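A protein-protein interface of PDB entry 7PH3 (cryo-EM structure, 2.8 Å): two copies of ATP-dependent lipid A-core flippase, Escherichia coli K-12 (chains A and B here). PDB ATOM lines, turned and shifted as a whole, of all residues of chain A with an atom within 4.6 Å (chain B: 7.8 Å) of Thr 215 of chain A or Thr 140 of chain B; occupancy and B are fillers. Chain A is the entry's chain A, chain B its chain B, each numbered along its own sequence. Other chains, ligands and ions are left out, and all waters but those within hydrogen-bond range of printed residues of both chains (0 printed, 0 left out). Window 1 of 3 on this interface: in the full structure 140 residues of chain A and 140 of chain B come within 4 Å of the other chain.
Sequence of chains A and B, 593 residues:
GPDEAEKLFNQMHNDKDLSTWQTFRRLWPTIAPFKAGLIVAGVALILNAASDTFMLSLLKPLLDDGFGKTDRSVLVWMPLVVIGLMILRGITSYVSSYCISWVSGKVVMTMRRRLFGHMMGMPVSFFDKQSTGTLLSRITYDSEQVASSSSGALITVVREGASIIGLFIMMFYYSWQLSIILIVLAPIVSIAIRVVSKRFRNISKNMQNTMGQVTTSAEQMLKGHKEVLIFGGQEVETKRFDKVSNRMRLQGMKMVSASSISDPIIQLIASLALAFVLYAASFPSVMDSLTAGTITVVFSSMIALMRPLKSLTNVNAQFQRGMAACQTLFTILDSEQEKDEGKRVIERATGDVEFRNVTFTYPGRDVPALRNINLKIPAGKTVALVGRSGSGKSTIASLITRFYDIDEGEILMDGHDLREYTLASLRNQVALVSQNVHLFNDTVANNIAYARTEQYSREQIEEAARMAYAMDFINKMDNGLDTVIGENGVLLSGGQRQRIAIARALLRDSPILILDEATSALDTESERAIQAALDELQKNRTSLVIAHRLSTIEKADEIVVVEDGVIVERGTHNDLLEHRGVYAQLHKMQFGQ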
ATOM      1  N   GLY A 133     -34.210  22.354 -20.960  1.00  0.00           N
ATOM      2  CA  GLY A 133     -33.984  22.685 -22.357  1.00  0.00           C
ATOM      3  C   GLY A 133     -34.972  23.698 -22.905  1.00  0.00           C
ATOM      4  O   GLY A 133     -34.620  24.527 -23.740  1.00  0.00           O
ATOM      5  N   SER A 137     -33.905  27.244 -24.304  1.00  0.00           N
ATOM      6  CA  SER A 137     -34.288  27.645 -25.649  1.00  0.00           C
ATOM      7  C   SER A 137     -34.855  29.054 -25.660  1.00  0.00           C
ATOM      8  O   SER A 137     -34.546  29.837 -26.559  1.00  0.00           O
ATOM      9  CB  SER A 137     -35.298  26.662 -26.216  1.00  0.00           C
ATOM     10  OG  SER A 137     -34.843  25.346 -26.022  1.00  0.00           O
ATOM     11  N   THR A 140     -31.735  31.215 -25.545  1.00  0.00           N
ATOM     12  CA  THR A 140     -30.865  31.187 -26.720  1.00  0.00           C
ATOM     13  C   THR A 140     -31.621  31.491 -28.011  1.00  0.00           C
ATOM     14  O   THR A 140     -31.460  32.563 -28.606  1.00  0.00           O
ATOM     15  CB  THR A 140     -30.178  29.820 -26.810  1.00  0.00           C
ATOM     16  OG1 THR A 140     -29.653  29.464 -25.528  1.00  0.00           O
ATOM     17  CG2 THR A 140     -29.054  29.849 -27.823  1.00  0.00           C
ATOM     18  N   TYR A 141     -32.516  30.586 -28.403  1.00  0.00           N
ATOM     19  CA  TYR A 141     -33.104  30.620 -29.736  1.00  0.00           C
ATOM     20  C   TYR A 141     -34.051  31.799 -29.902  1.00  0.00           C
ATOM     21  O   TYR A 141     -33.962  32.540 -30.885  1.00  0.00           O
ATOM     22  CB  TYR A 141     -33.824  29.296 -29.994  1.00  0.00           C
ATOM     23  CG  TYR A 141     -34.603  29.218 -31.280  1.00  0.00           C
ATOM     24  CD1 TYR A 141     -33.973  28.951 -32.478  1.00  0.00           C
ATOM     25  CD2 TYR A 141     -35.978  29.387 -31.290  1.00  0.00           C
ATOM     26  CE1 TYR A 141     -34.683  28.869 -33.641  1.00  0.00           C
ATOM     27  CE2 TYR A 141     -36.692  29.310 -32.451  1.00  0.00           C
ATOM     28  CZ  TYR A 141     -36.041  29.049 -33.624  1.00  0.00           C
ATOM     29  OH  TYR A 141     -36.754  28.963 -34.795  1.00  0.00           O
ATOM     30  N   MET A 211     -38.035  23.894 -31.334  1.00  0.00           N
ATOM     31  CA  MET A 211     -36.644  24.103 -30.955  1.00  0.00           C
ATOM     32  C   MET A 211     -36.440  23.841 -29.470  1.00  0.00           C
ATOM     33  O   MET A 211     -35.395  23.323 -29.060  1.00  0.00           O
ATOM     34  CB  MET A 211     -36.204  25.516 -31.313  1.00  0.00           C
ATOM     35  CG  MET A 211     -34.730  25.626 -31.559  1.00  0.00           C
ATOM     36  SD  MET A 211     -34.151  24.147 -32.390  1.00  0.00           S
ATOM     37  CE  MET A 211     -32.390  24.411 -32.370  1.00  0.00           C
ATOM     38  N   GLY A 212     -37.425  24.202 -28.651  1.00  0.00           N
ATOM     39  CA  GLY A 212     -37.386  23.798 -27.257  1.00  0.00           C
ATOM     40  C   GLY A 212     -37.307  22.294 -27.096  1.00  0.00           C
ATOM     41  O   GLY A 212     -36.570  21.787 -26.251  1.00  0.00           O
ATOM     42  N   GLN A 213     -38.058  21.558 -27.916  1.00  0.00           N
ATOM     43  CA  GLN A 213     -37.992  20.096 -27.870  1.00  0.00           C
ATOM     44  C   GLN A 213     -36.627  19.570 -28.304  1.00  0.00           C
ATOM     45  O   GLN A 213     -36.114  18.603 -27.731  1.00  0.00           O
ATOM     46  CB  GLN A 213     -39.084  19.498 -28.743  1.00  0.00           C
ATOM     47  CG  GLN A 213     -40.465  19.857 -28.308  1.00  0.00           C
ATOM     48  CD  GLN A 213     -41.482  18.900 -28.838  1.00  0.00           C
ATOM     49  OE1 GLN A 213     -41.447  18.533 -30.008  1.00  0.00           O
ATOM     50  NE2 GLN A 213     -42.400  18.477 -27.980  1.00  0.00           N
ATOM     51  N   VAL A 214     -36.038  20.180 -29.331  1.00  0.00           N
ATOM     52  CA  VAL A 214     -34.712  19.772 -29.796  1.00  0.00           C
ATOM     53  C   VAL A 214     -33.685  19.962 -28.689  1.00  0.00           C
ATOM     54  O   VAL A 214     -32.856  19.082 -28.415  1.00  0.00           O
ATOM     55  CB  VAL A 214     -34.322  20.564 -31.057  1.00  0.00           C
ATOM     56  CG1 VAL A 214     -32.883  20.296 -31.430  1.00  0.00           C
ATOM     57  CG2 VAL A 214     -35.233  20.230 -32.207  1.00  0.00           C
ATOM     58  N   THR A 215     -33.733  21.123 -28.038  1.00  0.00           N
ATOM     59  CA  THR A 215     -32.828  21.402 -26.932  1.00  0.00           C
ATOM     60  C   THR A 215     -33.054  20.441 -25.781  1.00  0.00           C
ATOM     61  O   THR A 215     -32.099  19.991 -25.150  1.00  0.00           O
ATOM     62  CB  THR A 215     -33.007  22.839 -26.465  1.00  0.00           C
ATOM     63  OG1 THR A 215     -33.134  23.698 -27.605  1.00  0.00           O
ATOM     64  CG2 THR A 215     -31.828  23.278 -25.620  1.00  0.00           C
ATOM     65  N   THR A 216     -34.314  20.132 -25.478  1.00  0.00           N
ATOM     66  CA  THR A 216     -34.607  19.187 -24.410  1.00  0.00           C
ATOM     67  C   THR A 216     -34.001  17.823 -24.702  1.00  0.00           C
ATOM     68  O   THR A 216     -33.418  17.192 -23.817  1.00  0.00           O
ATOM     69  CB  THR A 216     -36.118  19.079 -24.222  1.00  0.00           C
ATOM     70  OG1 THR A 216     -36.612  20.300 -23.664  1.00  0.00           O
ATOM     71  CG2 THR A 216     -36.478  17.928 -23.306  1.00  0.00           C
ATOM     72  N   SER A 217     -34.119  17.360 -25.946  1.00  0.00           N
ATOM     73  CA  SER A 217     -33.552  16.067 -26.316  1.00  0.00           C
ATOM     74  C   SER A 217     -32.034  16.065 -26.172  1.00  0.00           C
ATOM     75  O   SER A 217     -31.455  15.150 -25.571  1.00  0.00           O
ATOM     76  CB  SER A 217     -33.965  15.721 -27.745  1.00  0.00           C
ATOM     77  OG  SER A 217     -33.619  14.395 -28.073  1.00  0.00           O
ATOM     78  N   ALA A 218     -31.370  17.091 -26.711  1.00  0.00           N
ATOM     79  CA  ALA A 218     -29.912  17.148 -26.619  1.00  0.00           C
ATOM     80  C   ALA A 218     -29.447  17.263 -25.170  1.00  0.00           C
ATOM     81  O   ALA A 218     -28.476  16.615 -24.768  1.00  0.00           O
ATOM     82  CB  ALA A 218     -29.382  18.313 -27.451  1.00  0.00           C
ATOM     83  N   GLU A 219     -30.127  18.097 -24.381  1.00  0.00           N
ATOM     84  CA  GLU A 219     -29.878  18.218 -22.949  1.00  0.00           C
ATOM     85  C   GLU A 219     -29.981  16.880 -22.234  1.00  0.00           C
ATOM     86  O   GLU A 219     -29.075  16.499 -21.483  1.00  0.00           O
ATOM     87  CB  GLU A 219     -30.878  19.217 -22.367  1.00  0.00           C
ATOM     88  CG  GLU A 219     -30.889  19.390 -20.870  1.00  0.00           C
ATOM     89  CD  GLU A 219     -29.770  20.327 -20.417  1.00  0.00           C
ATOM     90  OE1 GLU A 219     -29.725  21.479 -20.906  1.00  0.00           O
ATOM     91  OE2 GLU A 219     -28.943  19.924 -19.569  1.00  0.00           O
ATOM     92  N   ARG B 112     -27.105  18.372 -38.036  1.00  0.00           N
ATOM     93  CA  ARG B 112     -27.560  18.313 -36.655  1.00  0.00           C
ATOM     94  C   ARG B 112     -27.533  16.888 -36.125  1.00  0.00           C
ATOM     95  O   ARG B 112     -27.097  16.643 -34.994  1.00  0.00           O
ATOM     96  CB  ARG B 112     -28.965  18.899 -36.565  1.00  0.00           C
ATOM     97  CG  ARG B 112     -28.993  20.328 -36.125  1.00  0.00           C
ATOM     98  CD  ARG B 112     -30.322  20.681 -35.515  1.00  0.00           C
ATOM     99  NE  ARG B 112     -31.187  21.340 -36.481  1.00  0.00           N
ATOM    100  CZ  ARG B 112     -31.360  22.651 -36.543  1.00  0.00           C
ATOM    101  NH1 ARG B 112     -32.165  23.168 -37.455  1.00  0.00           N
ATOM    102  NH2 ARG B 112     -30.734  23.441 -35.691  1.00  0.00           N
ATOM    103  N   LEU B 115     -23.933  15.868 -35.545  1.00  0.00           N
ATOM    104  CA  LEU B 115     -23.361  16.473 -34.347  1.00  0.00           C
ATOM    105  C   LEU B 115     -23.884  15.798 -33.086  1.00  0.00           C
ATOM    106  O   LEU B 115     -23.126  15.568 -32.135  1.00  0.00           O
ATOM    107  CB  LEU B 115     -23.647  17.974 -34.330  1.00  0.00           C
ATOM    108  CG  LEU B 115     -23.166  18.732 -33.093  1.00  0.00           C
ATOM    109  CD1 LEU B 115     -21.671  18.664 -32.987  1.00  0.00           C
ATOM    110  CD2 LEU B 115     -23.572  20.167 -33.145  1.00  0.00           C
ATOM    111  N   PHE B 116     -25.172  15.452 -33.068  1.00  0.00           N
ATOM    112  CA  PHE B 116     -25.725  14.717 -31.938  1.00  0.00           C
ATOM    113  C   PHE B 116     -25.040  13.364 -31.773  1.00  0.00           C
ATOM    114  O   PHE B 116     -24.660  12.978 -30.661  1.00  0.00           O
ATOM    115  CB  PHE B 116     -27.231  14.551 -32.129  1.00  0.00           C
ATOM    116  CG  PHE B 116     -27.932  13.912 -30.972  1.00  0.00           C
ATOM    117  CD1 PHE B 116     -28.429  14.679 -29.943  1.00  0.00           C
ATOM    118  CD2 PHE B 116     -28.112  12.542 -30.923  1.00  0.00           C
ATOM    119  CE1 PHE B 116     -29.078  14.099 -28.895  1.00  0.00           C
ATOM    120  CE2 PHE B 116     -28.754  11.964 -29.873  1.00  0.00           C
ATOM    121  CZ  PHE B 116     -29.242  12.743 -28.860  1.00  0.00           C
ATOM    122  N   GLY B 133     -23.589  23.672 -21.372  1.00  0.00           N
ATOM    123  CA  GLY B 133     -24.094  24.798 -22.143  1.00  0.00           C
ATOM    124  C   GLY B 133     -23.346  25.022 -23.443  1.00  0.00           C
ATOM    125  O   GLY B 133     -23.938  25.426 -24.441  1.00  0.00           O
ATOM    126  N   THR B 134     -22.040  24.765 -23.448  1.00  0.00           N
ATOM    127  CA  THR B 134     -21.242  24.933 -24.660  1.00  0.00           C
ATOM    128  C   THR B 134     -21.704  23.987 -25.767  1.00  0.00           C
ATOM    129  O   THR B 134     -21.937  24.407 -26.909  1.00  0.00           O
ATOM    130  CB  THR B 134     -19.769  24.700 -24.331  1.00  0.00           C
ATOM    131  OG1 THR B 134     -19.221  25.873 -23.723  1.00  0.00           O
ATOM    132  CG2 THR B 134     -18.976  24.356 -25.583  1.00  0.00           C
ATOM    133  N   LEU B 135     -21.839  22.699 -25.443  1.00  0.00           N
ATOM    134  CA  LEU B 135     -22.291  21.725 -26.428  1.00  0.00           C
ATOM    135  C   LEU B 135     -23.728  21.989 -26.846  1.00  0.00           C
ATOM    136  O   LEU B 135     -24.075  21.879 -28.032  1.00  0.00           O
ATOM    137  CB  LEU B 135     -22.136  20.317 -25.863  1.00  0.00           C
ATOM    138  CG  LEU B 135     -20.847  20.062 -25.073  1.00  0.00           C
ATOM    139  CD1 LEU B 135     -21.048  18.959 -24.057  1.00  0.00           C
ATOM    140  CD2 LEU B 135     -19.694  19.731 -25.993  1.00  0.00           C
ATOM    141  N   LEU B 136     -24.581  22.343 -25.889  1.00  0.00           N
ATOM    142  CA  LEU B 136     -25.952  22.673 -26.237  1.00  0.00           C
ATOM    143  C   LEU B 136     -26.005  23.879 -27.157  1.00  0.00           C
ATOM    144  O   LEU B 136     -26.893  23.973 -28.005  1.00  0.00           O
ATOM    145  CB  LEU B 136     -26.773  22.921 -24.975  1.00  0.00           C
ATOM    146  CG  LEU B 136     -26.938  21.693 -24.087  1.00  0.00           C
ATOM    147  CD1 LEU B 136     -27.635  22.062 -22.798  1.00  0.00           C
ATOM    148  CD2 LEU B 136     -27.678  20.591 -24.806  1.00  0.00           C
ATOM    149  N   SER B 137     -25.066  24.811 -27.003  1.00  0.00           N
ATOM    150  CA  SER B 137     -24.973  25.932 -27.927  1.00  0.00           C
ATOM    151  C   SER B 137     -24.595  25.465 -29.321  1.00  0.00           C
ATOM    152  O   SER B 137     -25.147  25.950 -30.308  1.00  0.00           O
ATOM    153  CB  SER B 137     -23.967  26.947 -27.413  1.00  0.00           C
ATOM    154  OG  SER B 137     -24.217  27.225 -26.058  1.00  0.00           O
ATOM    155  N   ARG B 138     -23.663  24.520 -29.421  1.00  0.00           N
ATOM    156  CA  ARG B 138     -23.357  23.941 -30.724  1.00  0.00           C
ATOM    157  C   ARG B 138     -24.608  23.369 -31.379  1.00  0.00           C
ATOM    158  O   ARG B 138     -24.819  23.537 -32.584  1.00  0.00           O
ATOM    159  CB  ARG B 138     -22.285  22.863 -30.586  1.00  0.00           C
ATOM    160  CG  ARG B 138     -20.884  23.332 -30.877  1.00  0.00           C
ATOM    161  CD  ARG B 138     -20.308  24.082 -29.704  1.00  0.00           C
ATOM    162  NE  ARG B 138     -18.851  24.164 -29.727  1.00  0.00           N
ATOM    163  CZ  ARG B 138     -18.157  24.919 -30.569  1.00  0.00           C
ATOM    164  NH1 ARG B 138     -18.774  25.593 -31.527  1.00  0.00           N
ATOM    165  NH2 ARG B 138     -16.840  24.998 -30.455  1.00  0.00           N
ATOM    166  N   ILE B 139     -25.454  22.693 -30.600  1.00  0.00           N
ATOM    167  CA  ILE B 139     -26.666  22.101 -31.174  1.00  0.00           C
ATOM    168  C   ILE B 139     -27.668  23.183 -31.567  1.00  0.00           C
ATOM    169  O   ILE B 139     -28.275  23.124 -32.640  1.00  0.00           O
ATOM    170  CB  ILE B 139     -27.294  21.088 -30.201  1.00  0.00           C
ATOM    171  CG1 ILE B 139     -26.298  20.000 -29.832  1.00  0.00           C
ATOM    172  CG2 ILE B 139     -28.502  20.423 -30.832  1.00  0.00           C
ATOM    173  CD1 ILE B 139     -25.790  19.235 -31.008  1.00  0.00           C
ATOM    174  N   THR B 140     -27.885  24.166 -30.698  1.00  0.00           N
ATOM    175  CA  THR B 140     -28.937  25.151 -30.944  1.00  0.00           C
ATOM    176  C   THR B 140     -28.461  26.303 -31.826  1.00  0.00           C
ATOM    177  O   THR B 140     -28.851  26.415 -32.992  1.00  0.00           O
ATOM    178  CB  THR B 140     -29.458  25.681 -29.604  1.00  0.00           C
ATOM    179  OG1 THR B 140     -29.704  24.584 -28.719  1.00  0.00           O
ATOM    180  CG2 THR B 140     -30.736  26.468 -29.797  1.00  0.00           C
ATOM    181  N   TYR B 141     -27.544  27.115 -31.300  1.00  0.00           N
ATOM    182  CA  TYR B 141     -27.206  28.389 -31.919  1.00  0.00           C
ATOM    183  C   TYR B 141     -26.453  28.195 -33.228  1.00  0.00           C
ATOM    184  O   TYR B 141     -26.802  28.798 -34.245  1.00  0.00           O
ATOM    185  CB  TYR B 141     -26.387  29.218 -30.931  1.00  0.00           C
ATOM    186  CG  TYR B 141     -25.840  30.516 -31.465  1.00  0.00           C
ATOM    187  CD1 TYR B 141     -26.634  31.643 -31.543  1.00  0.00           C
ATOM    188  CD2 TYR B 141     -24.519  30.619 -31.869  1.00  0.00           C
ATOM    189  CE1 TYR B 141     -26.132  32.822 -32.018  1.00  0.00           C
ATOM    190  CE2 TYR B 141     -24.015  31.794 -32.348  1.00  0.00           C
ATOM    191  CZ  TYR B 141     -24.824  32.893 -32.418  1.00  0.00           C
ATOM    192  OH  TYR B 141     -24.321  34.080 -32.892  1.00  0.00           O
ATOM    193  N   ASP B 142     -25.421  27.351 -33.219  1.00  0.00           N
ATOM    194  CA  ASP B 142     -24.557  27.205 -34.386  1.00  0.00           C
ATOM    195  C   ASP B 142     -25.322  26.631 -35.572  1.00  0.00           C
ATOM    196  O   ASP B 142     -25.260  27.161 -36.690  1.00  0.00           O
ATOM    197  CB  ASP B 142     -23.372  26.311 -34.033  1.00  0.00           C
ATOM    198  CG  ASP B 142     -22.387  26.979 -33.098  1.00  0.00           C
ATOM    199  OD1 ASP B 142     -22.443  28.213 -32.931  1.00  0.00           O
ATOM    200  OD2 ASP B 142     -21.578  26.259 -32.492  1.00  0.00           O
ATOM    201  N   SER B 143     -26.064  25.549 -35.343  1.00  0.00           N
ATOM    202  CA  SER B 143     -26.839  24.954 -36.422  1.00  0.00           C
ATOM    203  C   SER B 143     -27.981  25.857 -36.863  1.00  0.00           C
ATOM    204  O   SER B 143     -28.341  25.849 -38.044  1.00  0.00           O
ATOM    205  CB  SER B 143     -27.376  23.592 -36.005  1.00  0.00           C
ATOM    206  OG  SER B 143     -26.321  22.685 -35.794  1.00  0.00           O
ATOM    207  N   GLU B 144     -28.617  26.626 -35.961  1.00  0.00           N
ATOM    208  CA  GLU B 144     -29.645  27.541 -36.423  1.00  0.00           C
ATOM    209  C   GLU B 144     -29.049  28.683 -37.234  1.00  0.00           C
ATOM    210  O   GLU B 144     -29.724  29.237 -38.101  1.00  0.00           O
ATOM    211  CB  GLU B 144     -30.459  28.087 -35.252  1.00  0.00           C
ATOM    212  CG  GLU B 144     -31.651  29.030 -35.588  1.00  0.00           C
ATOM    213  CD  GLU B 144     -32.855  28.444 -36.379  1.00  0.00           C
ATOM    214  OE1 GLU B 144     -33.299  27.346 -36.015  1.00  0.00           O
ATOM    215  OE2 GLU B 144     -33.344  28.996 -37.380  1.00  0.00           O
ATOM    216  N   GLN B 145     -27.749  29.057 -36.973  1.00  0.00           N
ATOM    217  CA  GLN B 145     -27.070  30.013 -37.843  1.00  0.00           C
ATOM    218  C   GLN B 145     -26.854  29.426 -39.227  1.00  0.00           C
ATOM    219  O   GLN B 145     -27.057  30.109 -40.236  1.00  0.00           O
ATOM    220  CB  GLN B 145     -25.730  30.445 -37.240  1.00  0.00           C
ATOM    221  CG  GLN B 145     -25.832  31.202 -35.939  1.00  0.00           C
ATOM    222  CD  GLN B 145     -26.824  32.327 -35.993  1.00  0.00           C
ATOM    223  OE1 GLN B 145     -27.263  32.730 -37.061  1.00  0.00           O
ATOM    224  NE2 GLN B 145     -27.221  32.816 -34.832  1.00  0.00           N
ATOM    225  N   VAL B 146     -26.435  28.162 -39.289  1.00  0.00           N
ATOM    226  CA  VAL B 146     -26.314  27.483 -40.579  1.00  0.00           C
ATOM    227  C   VAL B 146     -27.645  27.510 -41.316  1.00  0.00           C
ATOM    228  O   VAL B 146     -27.712  27.815 -42.511  1.00  0.00           O
ATOM    229  CB  VAL B 146     -25.825  26.041 -40.386  1.00  0.00           C
ATOM    230  CG1 VAL B 146     -25.688  25.351 -41.717  1.00  0.00           C
ATOM    231  CG2 VAL B 146     -24.529  26.028 -39.644  1.00  0.00           C
ATOM    232  N   ALA B 147     -28.722  27.182 -40.609  1.00  0.00           N
ATOM    233  CA  ALA B 147     -30.039  27.147 -41.229  1.00  0.00           C
ATOM    234  C   ALA B 147     -30.451  28.523 -41.738  1.00  0.00           C
ATOM    235  O   ALA B 147     -30.888  28.666 -42.884  1.00  0.00           O
ATOM    236  CB  ALA B 147     -31.064  26.606 -40.237  1.00  0.00           C
ATOM    237  N   MET B 211     -21.849  33.015 -27.229  1.00  0.00           N
ATOM    238  CA  MET B 211     -23.168  32.428 -27.034  1.00  0.00           C
ATOM    239  C   MET B 211     -23.076  31.146 -26.219  1.00  0.00           C
ATOM    240  O   MET B 211     -23.962  30.850 -25.410  1.00  0.00           O
ATOM    241  CB  MET B 211     -23.832  32.160 -28.378  1.00  0.00           C
ATOM    242  CG  MET B 211     -25.328  32.172 -28.305  1.00  0.00           C
ATOM    243  SD  MET B 211     -25.859  33.436 -27.150  1.00  0.00           S
ATOM    244  CE  MET B 211     -27.608  33.113 -27.069  1.00  0.00           C
ATOM    245  N   THR B 215     -25.141  30.571 -22.730  1.00  0.00           N
ATOM    246  CA  THR B 215     -25.866  29.347 -22.422  1.00  0.00           C
ATOM    247  C   THR B 215     -25.327  28.690 -21.166  1.00  0.00           C
ATOM    248  O   THR B 215     -26.095  28.175 -20.355  1.00  0.00           O
ATOM    249  CB  THR B 215     -25.784  28.384 -23.599  1.00  0.00           C
ATOM    250  OG1 THR B 215     -25.964  29.111 -24.820  1.00  0.00           O
ATOM    251  CG2 THR B 215     -26.842  27.307 -23.483  1.00  0.00           C
ATOM    252  N   GLU B 219     -27.657  27.974 -17.992  1.00  0.00           N
ATOM    253  CA  GLU B 219     -27.666  26.587 -17.538  1.00  0.00           C
ATOM    254  C   GLU B 219     -27.278  26.461 -16.073  1.00  0.00           C
ATOM    255  O   GLU B 219     -27.986  25.816 -15.290  1.00  0.00           O
ATOM    256  CB  GLU B 219     -26.709  25.785 -18.418  1.00  0.00           C
ATOM    257  CG  GLU B 219     -26.350  24.396 -17.960  1.00  0.00           C
ATOM    258  CD  GLU B 219     -27.575  23.481 -17.964  1.00  0.00           C
ATOM    259  OE1 GLU B 219     -28.463  23.682 -18.825  1.00  0.00           O
ATOM    260  OE2 GLU B 219     -27.650  22.560 -17.122  1.00  0.00           O
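The side-chain carboxylate (OE1) of Glu 219 of chain A sits close to the side-chain carboxylate (OE1) of Glu 219 of chain B (3.3 Å).
The backbone carbonyl oxygen (O) of Met 211 of chain B is in hydrogen-bond range of the side-chain hydroxyl (OG1) of Thr 215 of chain B, at 2.7 Å.
OG1 of Thr 215 of chain A lies within hydrogen-bond range of O of Met 211 of chain A, at 2.7 Å.
O of Leu 136 of chain B sits at hydrogen-bond distance from OG1 of Thr 140 of chain B (3.0 Å).
The side-chain hydroxyl of Ser 137 of chain A sits at hydrogen-bond distance from the side-chain hydroxyl of Thr 215 of chain A, 2.9 Å away.
The side-chain hydroxyl (OG) of Ser 137 of chain B is in hydrogen-bond range of the side-chain hydroxyl (OG1) of Thr 215 of chain B (2.9 Å).
CE of Met 211 of chain B touches CG2 of Thr 140 of chain A, 3.6 Å away.
OG1 of Thr 215 of chain B touches OG1 of Thr 140 of chain A (3.8 Å).
Glu 144 of chain B touches Tyr 141 of chain A (OE1 to CE1, 3.1 Å).
Met 211 of chain A touches Arg 112 of chain B (CE to NH2, 3.8 Å).
Thr 140 of chain B touches Met 211 of chain A (CG2 to CE, 3.7 Å).
Thr 140 of chain B touches Thr 215 of chain A (OG1 to OG1, 3.7 Å).
Ala 218 of chain A touches Phe 116 of chain B.
C of Ala 218 of chain A touches CD2 of Leu 136 of chain B (3.8 Å).
Glu 219 of chain A touches Leu 136 of chain B.
Printed residues of chain B within 4 Å of Thr 215 of chain A: Thr 140 (3.7 Å).
Thr 216 of chain A touches none of the printed residues of chain B.
Printed residues of chain B within 4 Å of Ala 218 of chain A: Phe 116 and Leu 136.
Of the printed residues of chain A, Thr 140 of chain B touches Met 211 and Thr 215.
Of the printed residues of chain A, Met 211 of chain B touches Thr 140.
The nearest residue of chain B that does not touch Thr 215 of chain A is Leu 136 of chain B (4.5 Å).
The nearest residue of chain A that does not touch Thr 140 of chain B is Tyr 141 of chain A (4.2 Å).
The nearest printed residue of chain A that does not touch Thr 215 of chain B is Thr 215 of chain A (6.8 Å).
Hydrophobic or aromatic side chains of chain A within 4 Å of the printed part of chain B: Tyr 141, Met 211 and Ala 218.
Hydrophobic or aromatic side chains of chain B within 4 Å of the printed part of chain A: Phe 116, Leu 136 and Met 211.
Thr 140 of chain A touches Met 211 of chain B, and with the chains exchanged Met 211 of chain A touches Thr 140 of chain B.
Thr 140 of chain A touches Thr 215 of chain B, and with the chains exchanged Thr 215 of chain A touches Thr 140 of chain B.
Glu 219 of chain A touches its own counterpart, Glu 219 of chain B.
Positions printed for both chains: 133, 137, 140, 141, 211, 215 and 219.
Of the 10 pairs that touch across the chains among the printed residues, 5 have their exchanged pair printed and touching as well.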
